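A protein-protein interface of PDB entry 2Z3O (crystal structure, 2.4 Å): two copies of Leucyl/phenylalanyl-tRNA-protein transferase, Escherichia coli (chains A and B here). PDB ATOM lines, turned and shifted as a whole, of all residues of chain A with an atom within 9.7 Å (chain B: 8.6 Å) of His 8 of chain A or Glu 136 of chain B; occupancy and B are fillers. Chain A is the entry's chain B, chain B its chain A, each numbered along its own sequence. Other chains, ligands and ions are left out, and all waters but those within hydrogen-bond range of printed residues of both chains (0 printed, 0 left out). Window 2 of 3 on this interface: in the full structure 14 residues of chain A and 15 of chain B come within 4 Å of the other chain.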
ATOM      1  N   GLN A   4       9.598 -18.121 -36.555  1.00  0.00           N
ATOM      2  CA  GLN A   4      11.027 -17.977 -36.297  1.00  0.00           C
ATOM      3  C   GLN A   4      11.354 -16.515 -36.035  1.00  0.00           C
ATOM      4  O   GLN A   4      11.173 -15.661 -36.892  1.00  0.00           O
ATOM      5  CB  GLN A   4      11.879 -18.479 -37.458  1.00  0.00           C
ATOM      6  CG  GLN A   4      13.366 -18.357 -37.150  1.00  0.00           C
ATOM      7  CD  GLN A   4      14.229 -19.057 -38.158  1.00  0.00           C
ATOM      8  OE1 GLN A   4      14.071 -20.256 -38.409  1.00  0.00           O
ATOM      9  NE2 GLN A   4      15.163 -18.315 -38.746  1.00  0.00           N
ATOM     10  N   LEU A   5      11.854 -16.241 -34.841  1.00  0.00           N
ATOM     11  CA  LEU A   5      12.191 -14.892 -34.434  1.00  0.00           C
ATOM     12  C   LEU A   5      13.447 -14.352 -35.113  1.00  0.00           C
ATOM     13  O   LEU A   5      14.097 -15.063 -35.890  1.00  0.00           O
ATOM     14  CB  LEU A   5      12.380 -14.881 -32.931  1.00  0.00           C
ATOM     15  CG  LEU A   5      11.336 -15.709 -32.196  1.00  0.00           C
ATOM     16  CD1 LEU A   5      11.773 -15.910 -30.761  1.00  0.00           C
ATOM     17  CD2 LEU A   5       9.977 -15.015 -32.291  1.00  0.00           C
ATOM     18  N   SER A   6      13.773 -13.089 -34.802  1.00  0.00           N
ATOM     19  CA  SER A   6      14.946 -12.393 -35.334  1.00  0.00           C
ATOM     20  C   SER A   6      15.349 -11.246 -34.406  1.00  0.00           C
ATOM     21  O   SER A   6      14.603 -10.890 -33.490  1.00  0.00           O
ATOM     22  CB  SER A   6      14.653 -11.800 -36.709  1.00  0.00           C
ATOM     23  OG  SER A   6      14.328 -10.428 -36.589  1.00  0.00           O
ATOM     24  N   ARG A   7      16.516 -10.659 -34.660  1.00  0.00           N
ATOM     25  CA  ARG A   7      17.012  -9.551 -33.844  1.00  0.00           C
ATOM     26  C   ARG A   7      16.177  -8.297 -34.092  1.00  0.00           C
ATOM     27  O   ARG A   7      16.193  -7.344 -33.307  1.00  0.00           O
ATOM     28  CB  ARG A   7      18.478  -9.275 -34.177  1.00  0.00           C
ATOM     29  CG  ARG A   7      19.216  -8.467 -33.119  1.00  0.00           C
ATOM     30  CD  ARG A   7      20.743  -8.547 -33.284  1.00  0.00           C
ATOM     31  NE  ARG A   7      21.426  -7.807 -32.224  1.00  0.00           N
ATOM     32  CZ  ARG A   7      22.389  -6.909 -32.427  1.00  0.00           C
ATOM     33  NH1 ARG A   7      22.805  -6.627 -33.663  1.00  0.00           N
ATOM     34  NH2 ARG A   7      22.926  -6.275 -31.388  1.00  0.00           N
ATOM     35  N   HIS A   8      15.427  -8.324 -35.183  1.00  0.00           N
ATOM     36  CA  HIS A   8      14.587  -7.208 -35.564  1.00  0.00           C
ATOM     37  C   HIS A   8      13.391  -6.983 -34.650  1.00  0.00           C
ATOM     38  O   HIS A   8      12.866  -5.872 -34.576  1.00  0.00           O
ATOM     39  CB  HIS A   8      14.120  -7.396 -37.007  1.00  0.00           C
ATOM     40  CG  HIS A   8      15.243  -7.446 -37.994  1.00  0.00           C
ATOM     41  ND1 HIS A   8      15.048  -7.698 -39.334  1.00  0.00           N
ATOM     42  CD2 HIS A   8      16.577  -7.273 -37.835  1.00  0.00           C
ATOM     43  CE1 HIS A   8      16.213  -7.678 -39.958  1.00  0.00           C
ATOM     44  NE2 HIS A   8      17.158  -7.422 -39.072  1.00  0.00           N
ATOM     45  N   SER A   9      12.954  -8.022 -33.948  1.00  0.00           N
ATOM     46  CA  SER A   9      11.818  -7.858 -33.051  1.00  0.00           C
ATOM     47  C   SER A   9      11.815  -8.780 -31.842  1.00  0.00           C
ATOM     48  O   SER A   9      12.178  -9.949 -31.924  1.00  0.00           O
ATOM     49  CB  SER A   9      10.509  -8.036 -33.814  1.00  0.00           C
ATOM     50  OG  SER A   9       9.409  -7.850 -32.938  1.00  0.00           O
ATOM     51  N   ILE A  10      11.378  -8.224 -30.723  1.00  0.00           N
ATOM     52  CA  ILE A  10      11.293  -8.929 -29.457  1.00  0.00           C
ATOM     53  C   ILE A  10       9.858  -9.398 -29.214  1.00  0.00           C
ATOM     54  O   ILE A  10       9.462  -9.694 -28.086  1.00  0.00           O
ATOM     55  CB  ILE A  10      11.751  -7.987 -28.324  1.00  0.00           C
ATOM     56  CG1 ILE A  10      10.578  -7.109 -27.917  1.00  0.00           C
ATOM     57  CG2 ILE A  10      12.893  -7.108 -28.759  1.00  0.00           C
ATOM     58  CD1 ILE A  10      10.811  -6.186 -26.710  1.00  0.00           C
ATOM     59  N   ALA A  11       9.085  -9.481 -30.289  1.00  0.00           N
ATOM     60  CA  ALA A  11       7.693  -9.890 -30.176  1.00  0.00           C
ATOM     61  C   ALA A  11       7.472 -11.362 -30.499  1.00  0.00           C
ATOM     62  O   ALA A  11       7.971 -11.876 -31.508  1.00  0.00           O
ATOM     63  CB  ALA A  11       6.823  -9.019 -31.085  1.00  0.00           C
ATOM     64  N   GLY A  29      14.618 -19.316 -32.454  1.00  0.00           N
ATOM     65  CA  GLY A  29      15.534 -18.273 -32.873  1.00  0.00           C
ATOM     66  C   GLY A  29      15.574 -17.124 -31.887  1.00  0.00           C
ATOM     67  O   GLY A  29      15.288 -17.312 -30.709  1.00  0.00           O
ATOM     68  N   GLY A  30      15.915 -15.932 -32.370  1.00  0.00           N
ATOM     69  CA  GLY A  30      16.003 -14.771 -31.503  1.00  0.00           C
ATOM     70  C   GLY A  30      17.278 -14.860 -30.682  1.00  0.00           C
ATOM     71  O   GLY A  30      18.286 -15.405 -31.144  1.00  0.00           O
ATOM     72  N   ASP A  31      17.237 -14.327 -29.466  1.00  0.00           N
ATOM     73  CA  ASP A  31      18.381 -14.361 -28.569  1.00  0.00           C
ATOM     74  C   ASP A  31      17.857 -14.466 -27.138  1.00  0.00           C
ATOM     75  O   ASP A  31      16.660 -14.657 -26.930  1.00  0.00           O
ATOM     76  CB  ASP A  31      19.227 -13.093 -28.734  1.00  0.00           C
ATOM     77  CG  ASP A  31      18.430 -11.820 -28.494  1.00  0.00           C
ATOM     78  OD1 ASP A  31      17.884 -11.669 -27.373  1.00  0.00           O
ATOM     79  OD2 ASP A  31      18.346 -10.968 -29.420  1.00  0.00           O
ATOM     80  N   SER A  33      18.460 -11.976 -24.796  1.00  0.00           N
ATOM     81  CA  SER A  33      18.642 -10.623 -24.266  1.00  0.00           C
ATOM     82  C   SER A  33      17.658 -10.386 -23.131  1.00  0.00           C
ATOM     83  O   SER A  33      16.565 -10.955 -23.124  1.00  0.00           O
ATOM     84  CB  SER A  33      18.430  -9.552 -25.358  1.00  0.00           C
ATOM     85  OG  SER A  33      17.135  -9.619 -25.956  1.00  0.00           O
ATOM     86  N   PRO A  34      18.034  -9.539 -22.159  1.00  0.00           N
ATOM     87  CA  PRO A  34      17.168  -9.239 -21.013  1.00  0.00           C
ATOM     88  C   PRO A  34      15.777  -8.865 -21.482  1.00  0.00           C
ATOM     89  O   PRO A  34      14.776  -9.350 -20.953  1.00  0.00           O
ATOM     90  CB  PRO A  34      17.874  -8.066 -20.337  1.00  0.00           C
ATOM     91  CG  PRO A  34      19.300  -8.284 -20.667  1.00  0.00           C
ATOM     92  CD  PRO A  34      19.278  -8.752 -22.101  1.00  0.00           C
ATOM     93  N   ALA A  35      15.732  -8.011 -22.495  1.00  0.00           N
ATOM     94  CA  ALA A  35      14.475  -7.533 -23.050  1.00  0.00           C
ATOM     95  C   ALA A  35      13.607  -8.647 -23.601  1.00  0.00           C
ATOM     96  O   ALA A  35      12.420  -8.739 -23.268  1.00  0.00           O
ATOM     97  CB  ALA A  35      14.746  -6.490 -24.148  1.00  0.00           C
ATOM     98  N   ARG A  36      14.182  -9.495 -24.444  1.00  0.00           N
ATOM     99  CA  ARG A  36      13.398 -10.574 -25.028  1.00  0.00           C
ATOM    100  C   ARG A  36      12.856 -11.544 -23.977  1.00  0.00           C
ATOM    101  O   ARG A  36      11.720 -11.992 -24.074  1.00  0.00           O
ATOM    102  CB  ARG A  36      14.214 -11.338 -26.068  1.00  0.00           C
ATOM    103  CG  ARG A  36      13.384 -12.369 -26.775  1.00  0.00           C
ATOM    104  CD  ARG A  36      14.164 -13.153 -27.790  1.00  0.00           C
ATOM    105  NE  ARG A  36      13.863 -12.693 -29.137  1.00  0.00           N
ATOM    106  CZ  ARG A  36      14.598 -11.817 -29.803  1.00  0.00           C
ATOM    107  NH1 ARG A  36      15.686 -11.307 -29.238  1.00  0.00           N
ATOM    108  NH2 ARG A  36      14.241 -11.460 -31.028  1.00  0.00           N
ATOM    109  N   LEU A  37      13.662 -11.858 -22.971  1.00  0.00           N
ATOM    110  CA  LEU A  37      13.225 -12.769 -21.923  1.00  0.00           C
ATOM    111  C   LEU A  37      12.092 -12.163 -21.104  1.00  0.00           C
ATOM    112  O   LEU A  37      11.080 -12.816 -20.843  1.00  0.00           O
ATOM    113  CB  LEU A  37      14.398 -13.145 -21.006  1.00  0.00           C
ATOM    114  CG  LEU A  37      15.401 -14.136 -21.600  1.00  0.00           C
ATOM    115  CD1 LEU A  37      16.390 -14.551 -20.539  1.00  0.00           C
ATOM    116  CD2 LEU A  37      14.672 -15.359 -22.157  1.00  0.00           C
ATOM    117  N   MET A  39      10.021  -9.974 -22.012  1.00  0.00           N
ATOM    118  CA  MET A  39       8.837  -9.944 -22.862  1.00  0.00           C
ATOM    119  C   MET A  39       8.204 -11.338 -22.900  1.00  0.00           C
ATOM    120  O   MET A  39       6.978 -11.488 -22.863  1.00  0.00           O
ATOM    121  CB  MET A  39       9.211  -9.495 -24.273  1.00  0.00           C
ATOM    122  CG  MET A  39       9.474  -7.994 -24.406  1.00  0.00           C
ATOM    123  SD  MET A  39       7.961  -6.990 -24.266  1.00  0.00           S
ATOM    124  CE  MET A  39       8.390  -5.851 -22.989  1.00  0.00           C
ATOM    125  N   PRO B  85       9.008   3.722 -33.531  1.00  0.00           N
ATOM    126  CA  PRO B  85       9.800   2.506 -33.731  1.00  0.00           C
ATOM    127  C   PRO B  85      10.389   2.084 -32.381  1.00  0.00           C
ATOM    128  O   PRO B  85      11.271   1.239 -32.309  1.00  0.00           O
ATOM    129  CB  PRO B  85      10.884   2.977 -34.680  1.00  0.00           C
ATOM    130  CG  PRO B  85      11.201   4.342 -34.098  1.00  0.00           C
ATOM    131  CD  PRO B  85       9.818   4.921 -33.822  1.00  0.00           C
ATOM    132  N   TYR B  86       9.899   2.687 -31.310  1.00  0.00           N
ATOM    133  CA  TYR B  86      10.417   2.401 -29.977  1.00  0.00           C
ATOM    134  C   TYR B  86       9.431   1.724 -29.039  1.00  0.00           C
ATOM    135  O   TYR B  86       8.211   1.827 -29.174  1.00  0.00           O
ATOM    136  CB  TYR B  86      10.898   3.698 -29.308  1.00  0.00           C
ATOM    137  CG  TYR B  86      12.050   4.389 -30.003  1.00  0.00           C
ATOM    138  CD1 TYR B  86      12.037   5.769 -30.198  1.00  0.00           C
ATOM    139  CD2 TYR B  86      13.149   3.667 -30.474  1.00  0.00           C
ATOM    140  CE1 TYR B  86      13.098   6.423 -30.856  1.00  0.00           C
ATOM    141  CE2 TYR B  86      14.213   4.302 -31.132  1.00  0.00           C
ATOM    142  CZ  TYR B  86      14.179   5.681 -31.322  1.00  0.00           C
ATOM    143  OH  TYR B  86      15.193   6.315 -32.005  1.00  0.00           O
ATOM    144  N   ARG B  87       9.990   1.019 -28.074  1.00  0.00           N
ATOM    145  CA  ARG B  87       9.193   0.355 -27.060  1.00  0.00           C
ATOM    146  C   ARG B  87       9.613   1.016 -25.739  1.00  0.00           C
ATOM    147  O   ARG B  87      10.773   1.353 -25.549  1.00  0.00           O
ATOM    148  CB  ARG B  87       9.501  -1.148 -27.068  1.00  0.00           C
ATOM    149  CG  ARG B  87       8.648  -1.988 -26.139  1.00  0.00           C
ATOM    150  CD  ARG B  87       8.810  -3.495 -26.427  1.00  0.00           C
ATOM    151  NE  ARG B  87       7.852  -3.998 -27.420  1.00  0.00           N
ATOM    152  CZ  ARG B  87       8.159  -4.379 -28.662  1.00  0.00           C
ATOM    153  NH1 ARG B  87       9.416  -4.318 -29.101  1.00  0.00           N
ATOM    154  NH2 ARG B  87       7.207  -4.842 -29.468  1.00  0.00           N
ATOM    155  N   VAL B 133      13.926   2.786 -23.058  1.00  0.00           N
ATOM    156  CA  VAL B 133      13.435   2.917 -24.414  1.00  0.00           C
ATOM    157  C   VAL B 133      14.172   1.888 -25.249  1.00  0.00           C
ATOM    158  O   VAL B 133      15.400   1.921 -25.337  1.00  0.00           O
ATOM    159  CB  VAL B 133      13.692   4.312 -24.988  1.00  0.00           C
ATOM    160  CG1 VAL B 133      13.219   4.363 -26.440  1.00  0.00           C
ATOM    161  CG2 VAL B 133      12.960   5.343 -24.159  1.00  0.00           C
ATOM    162  N   TRP B 134      13.410   0.974 -25.853  1.00  0.00           N
ATOM    163  CA  TRP B 134      13.967  -0.091 -26.667  1.00  0.00           C
ATOM    164  C   TRP B 134      13.699   0.068 -28.157  1.00  0.00           C
ATOM    165  O   TRP B 134      12.602   0.444 -28.584  1.00  0.00           O
ATOM    166  CB  TRP B 134      13.408  -1.469 -26.247  1.00  0.00           C
ATOM    167  CG  TRP B 134      13.520  -1.786 -24.789  1.00  0.00           C
ATOM    168  CD1 TRP B 134      12.569  -1.572 -23.821  1.00  0.00           C
ATOM    169  CD2 TRP B 134      14.665  -2.319 -24.117  1.00  0.00           C
ATOM    170  NE1 TRP B 134      13.059  -1.939 -22.590  1.00  0.00           N
ATOM    171  CE2 TRP B 134      14.343  -2.395 -22.741  1.00  0.00           C
ATOM    172  CE3 TRP B 134      15.937  -2.736 -24.542  1.00  0.00           C
ATOM    173  CZ2 TRP B 134      15.249  -2.866 -21.785  1.00  0.00           C
ATOM    174  CZ3 TRP B 134      16.841  -3.207 -23.589  1.00  0.00           C
ATOM    175  CH2 TRP B 134      16.488  -3.265 -22.222  1.00  0.00           C
ATOM    176  N   ARG B 135      14.726  -0.238 -28.939  1.00  0.00           N
ATOM    177  CA  ARG B 135      14.621  -0.224 -30.384  1.00  0.00           C
ATOM    178  C   ARG B 135      14.900  -1.669 -30.724  1.00  0.00           C
ATOM    179  O   ARG B 135      16.040  -2.114 -30.645  1.00  0.00           O
ATOM    180  CB  ARG B 135      15.679   0.672 -31.017  1.00  0.00           C
ATOM    181  CG  ARG B 135      15.676   0.590 -32.528  1.00  0.00           C
ATOM    182  CD  ARG B 135      14.251   0.733 -33.101  1.00  0.00           C
ATOM    183  NE  ARG B 135      14.276   0.455 -34.525  1.00  0.00           N
ATOM    184  CZ  ARG B 135      13.262  -0.023 -35.232  1.00  0.00           C
ATOM    185  NH1 ARG B 135      12.096  -0.286 -34.659  1.00  0.00           N
ATOM    186  NH2 ARG B 135      13.439  -0.270 -36.514  1.00  0.00           N
ATOM    187  N   GLU B 136      13.856  -2.405 -31.082  1.00  0.00           N
ATOM    188  CA  GLU B 136      14.002  -3.822 -31.395  1.00  0.00           C
ATOM    189  C   GLU B 136      14.402  -4.489 -30.081  1.00  0.00           C
ATOM    190  O   GLU B 136      13.681  -4.410 -29.085  1.00  0.00           O
ATOM    191  CB  GLU B 136      15.107  -4.057 -32.445  1.00  0.00           C
ATOM    192  CG  GLU B 136      14.948  -3.280 -33.759  1.00  0.00           C
ATOM    193  CD  GLU B 136      16.010  -3.641 -34.820  1.00  0.00           C
ATOM    194  OE1 GLU B 136      17.225  -3.468 -34.550  1.00  0.00           O
ATOM    195  OE2 GLU B 136      15.629  -4.092 -35.928  1.00  0.00           O
ATOM    196  N   ASP B 137      15.574  -5.113 -30.085  1.00  0.00           N
ATOM    197  CA  ASP B 137      16.106  -5.806 -28.921  1.00  0.00           C
ATOM    198  C   ASP B 137      17.196  -4.990 -28.230  1.00  0.00           C
ATOM    199  O   ASP B 137      17.759  -5.447 -27.233  1.00  0.00           O
ATOM    200  CB  ASP B 137      16.693  -7.153 -29.348  1.00  0.00           C
ATOM    201  CG  ASP B 137      17.851  -6.996 -30.316  1.00  0.00           C
ATOM    202  OD1 ASP B 137      17.911  -5.958 -30.997  1.00  0.00           O
ATOM    203  OD2 ASP B 137      18.700  -7.908 -30.412  1.00  0.00           O
ATOM    204  N   GLU B 138      17.484  -3.795 -28.754  1.00  0.00           N
ATOM    205  CA  GLU B 138      18.532  -2.920 -28.198  1.00  0.00           C
ATOM    206  C   GLU B 138      18.015  -1.764 -27.337  1.00  0.00           C
ATOM    207  O   GLU B 138      17.018  -1.121 -27.668  1.00  0.00           O
ATOM    208  CB  GLU B 138      19.383  -2.337 -29.333  1.00  0.00           C
ATOM    209  CG  GLU B 138      20.717  -1.748 -28.891  1.00  0.00           C
ATOM    210  CD  GLU B 138      21.815  -2.809 -28.708  1.00  0.00           C
ATOM    211  OE1 GLU B 138      21.565  -3.875 -28.099  1.00  0.00           O
ATOM    212  OE2 GLU B 138      22.950  -2.570 -29.174  1.00  0.00           O
ATOM    213  N   LEU B 139      18.707  -1.508 -26.230  1.00  0.00           N
ATOM    214  CA  LEU B 139      18.359  -0.415 -25.319  1.00  0.00           C
ATOM    215  C   LEU B 139      18.929   0.857 -25.944  1.00  0.00           C
ATOM    216  O   LEU B 139      20.137   1.042 -25.974  1.00  0.00           O
ATOM    217  CB  LEU B 139      19.003  -0.640 -23.949  1.00  0.00           C
ATOM    218  CG  LEU B 139      18.773   0.477 -22.918  1.00  0.00           C
ATOM    219  CD1 LEU B 139      17.285   0.545 -22.545  1.00  0.00           C
ATOM    220  CD2 LEU B 139      19.634   0.233 -21.689  1.00  0.00           C
ATOM    221  N   VAL B 140      18.079   1.749 -26.423  1.00  0.00           N
ATOM    222  CA  VAL B 140      18.611   2.932 -27.070  1.00  0.00           C
ATOM    223  C   VAL B 140      18.415   4.237 -26.338  1.00  0.00           C
ATOM    224  O   VAL B 140      18.742   5.289 -26.869  1.00  0.00           O
ATOM    225  CB  VAL B 140      18.043   3.054 -28.477  1.00  0.00           C
ATOM    226  CG1 VAL B 140      18.474   1.842 -29.312  1.00  0.00           C
ATOM    227  CG2 VAL B 140      16.528   3.124 -28.406  1.00  0.00           C
ATOM    228  N   MET B 161      19.833   6.981 -29.854  1.00  0.00           N
ATOM    229  CA  MET B 161      19.102   7.004 -31.117  1.00  0.00           C
ATOM    230  C   MET B 161      18.095   8.160 -31.134  1.00  0.00           C
ATOM    231  O   MET B 161      17.465   8.459 -30.127  1.00  0.00           O
ATOM    232  CB  MET B 161      18.397   5.661 -31.330  1.00  0.00           C
ATOM    233  CG  MET B 161      18.033   5.350 -32.765  1.00  0.00           C
ATOM    234  SD  MET B 161      17.658   3.598 -32.932  1.00  0.00           S
ATOM    235  CE  MET B 161      16.295   3.634 -34.027  1.00  0.00           C
ATOM    236  N   PRO B 231       5.602  -0.424 -29.577  1.00  0.00           N
ATOM    237  CA  PRO B 231       5.648   0.143 -30.928  1.00  0.00           C
ATOM    238  C   PRO B 231       4.619  -0.524 -31.834  1.00  0.00           C
ATOM    239  O   PRO B 231       3.780  -1.304 -31.361  1.00  0.00           O
ATOM    240  CB  PRO B 231       7.084  -0.138 -31.372  1.00  0.00           C
ATOM    241  CG  PRO B 231       7.387  -1.437 -30.691  1.00  0.00           C
ATOM    242  CD  PRO B 231       6.822  -1.205 -29.299  1.00  0.00           C
ATOM    243  N   GLN B 232       4.678  -0.203 -33.126  1.00  0.00           N
ATOM    244  CA  GLN B 232       3.767  -0.782 -34.118  1.00  0.00           C
ATOM    245  C   GLN B 232       4.568  -1.499 -35.212  1.00  0.00           C
ATOM    246  O   GLN B 232       5.803  -1.317 -35.252  1.00  0.00           O
ATOM    247  CB  GLN B 232       2.890   0.314 -34.746  1.00  0.00           C
ATOM    248  CG  GLN B 232       1.826  -0.197 -35.723  1.00  0.00           C
ATOM    249  CD  GLN B 232       0.740  -1.036 -35.051  1.00  0.00           C
ATOM    250  OE1 GLN B 232      -0.186  -1.514 -35.712  1.00  0.00           O
ATOM    251  NE2 GLN B 232       0.850  -1.216 -33.733  1.00  0.00           N
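Printed residues of chain A that touch a printed residue of chain B: Arg 7, His 8, Ile 10, Asp 31 and Ala 35. Of the 14 printed residues of chain B, 4 touch a printed residue of chain A. Printed residues of chain B that touch a printed residue of chain A: Arg 87, Trp 134, Glu 136 and Asp 137. Hydrophobic or aromatic side chains of chain B that line the printed part of chain A: Trp 134.
No position is printed for both chains. Of the 8 pairs that touch across the chains among the printed residues, none has its exchanged pair printed and touching as well.
Of chain B, only Glu 136 comes within 4 Å of His 8 of chain A. Of chain A, only Arg 7, His 8 and Ile 10 come within 4 Å of Glu 136 of chain B. No residue of chain B comes within 4 Å of Ser 9 of chain A. No residue of chain A comes within 4 Å of Arg 135 of chain B. Asp 137 of chain B touches just these residues of chain A: Arg 7 (2.8 Å), Ile 10 (3.5 Å) and Asp 31 (3.2 Å). Of the printed residues of chain B, Ile 10 of chain A touches Arg 87, Glu 136 and Asp 137. Of the printed residues of chain B, Ala 35 of chain A touches Trp 134. The nearest residue of chain B that does not touch His 8 of chain A is Asp 137 of chain B (5.3 Å). The nearest printed residue of chain B that does not touch Asp 31 of chain A is Glu 138 of chain B (7.3 Å).
The backbone carbonyl oxygen (O) of Arg 87 of chain B sits at hydrogen-bond distance from the backbone NH (N) of Trp 134 of chain B, 2.7 Å away. The side-chain hydroxyl of Ser 6 of chain A lies within hydrogen-bond range of the backbone NH of His 8 of chain A, at 2.8 Å. OD1 of Asp 31 of chain A is in hydrogen-bond range of OG of Ser 33 of chain A (2.6 Å). The side-chain carboxylate of Asp 31 of chain A lies within salt-bridge range of the guanidinium group of Arg 36 of chain A (2.7 Å).
Among the printed residues, pairs that only touch across the chains: Arg 7 of chain A with Glu 136 of chain B (3.6 Å), His 8 of chain A with Glu 136 of chain B (3.3 Å), Ile 10 of chain A with Arg 87 of chain B (3.2 Å), Ile 10 of chain A with Glu 136 of chain B (2.8 Å), Ile 10 of chain A with Asp 137 of chain B (3.5 Å) and Ala 35 of chain A with Trp 134 of chain B (3.9 Å).
NE of Arg 7 of chain A lies within salt-bridge range of OD2 of Asp 137 of chain B (3.3 Å). The side-chain carboxylate of Asp 137 of chain B sits close to the side-chain carboxylate of Asp 31 of chain A.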
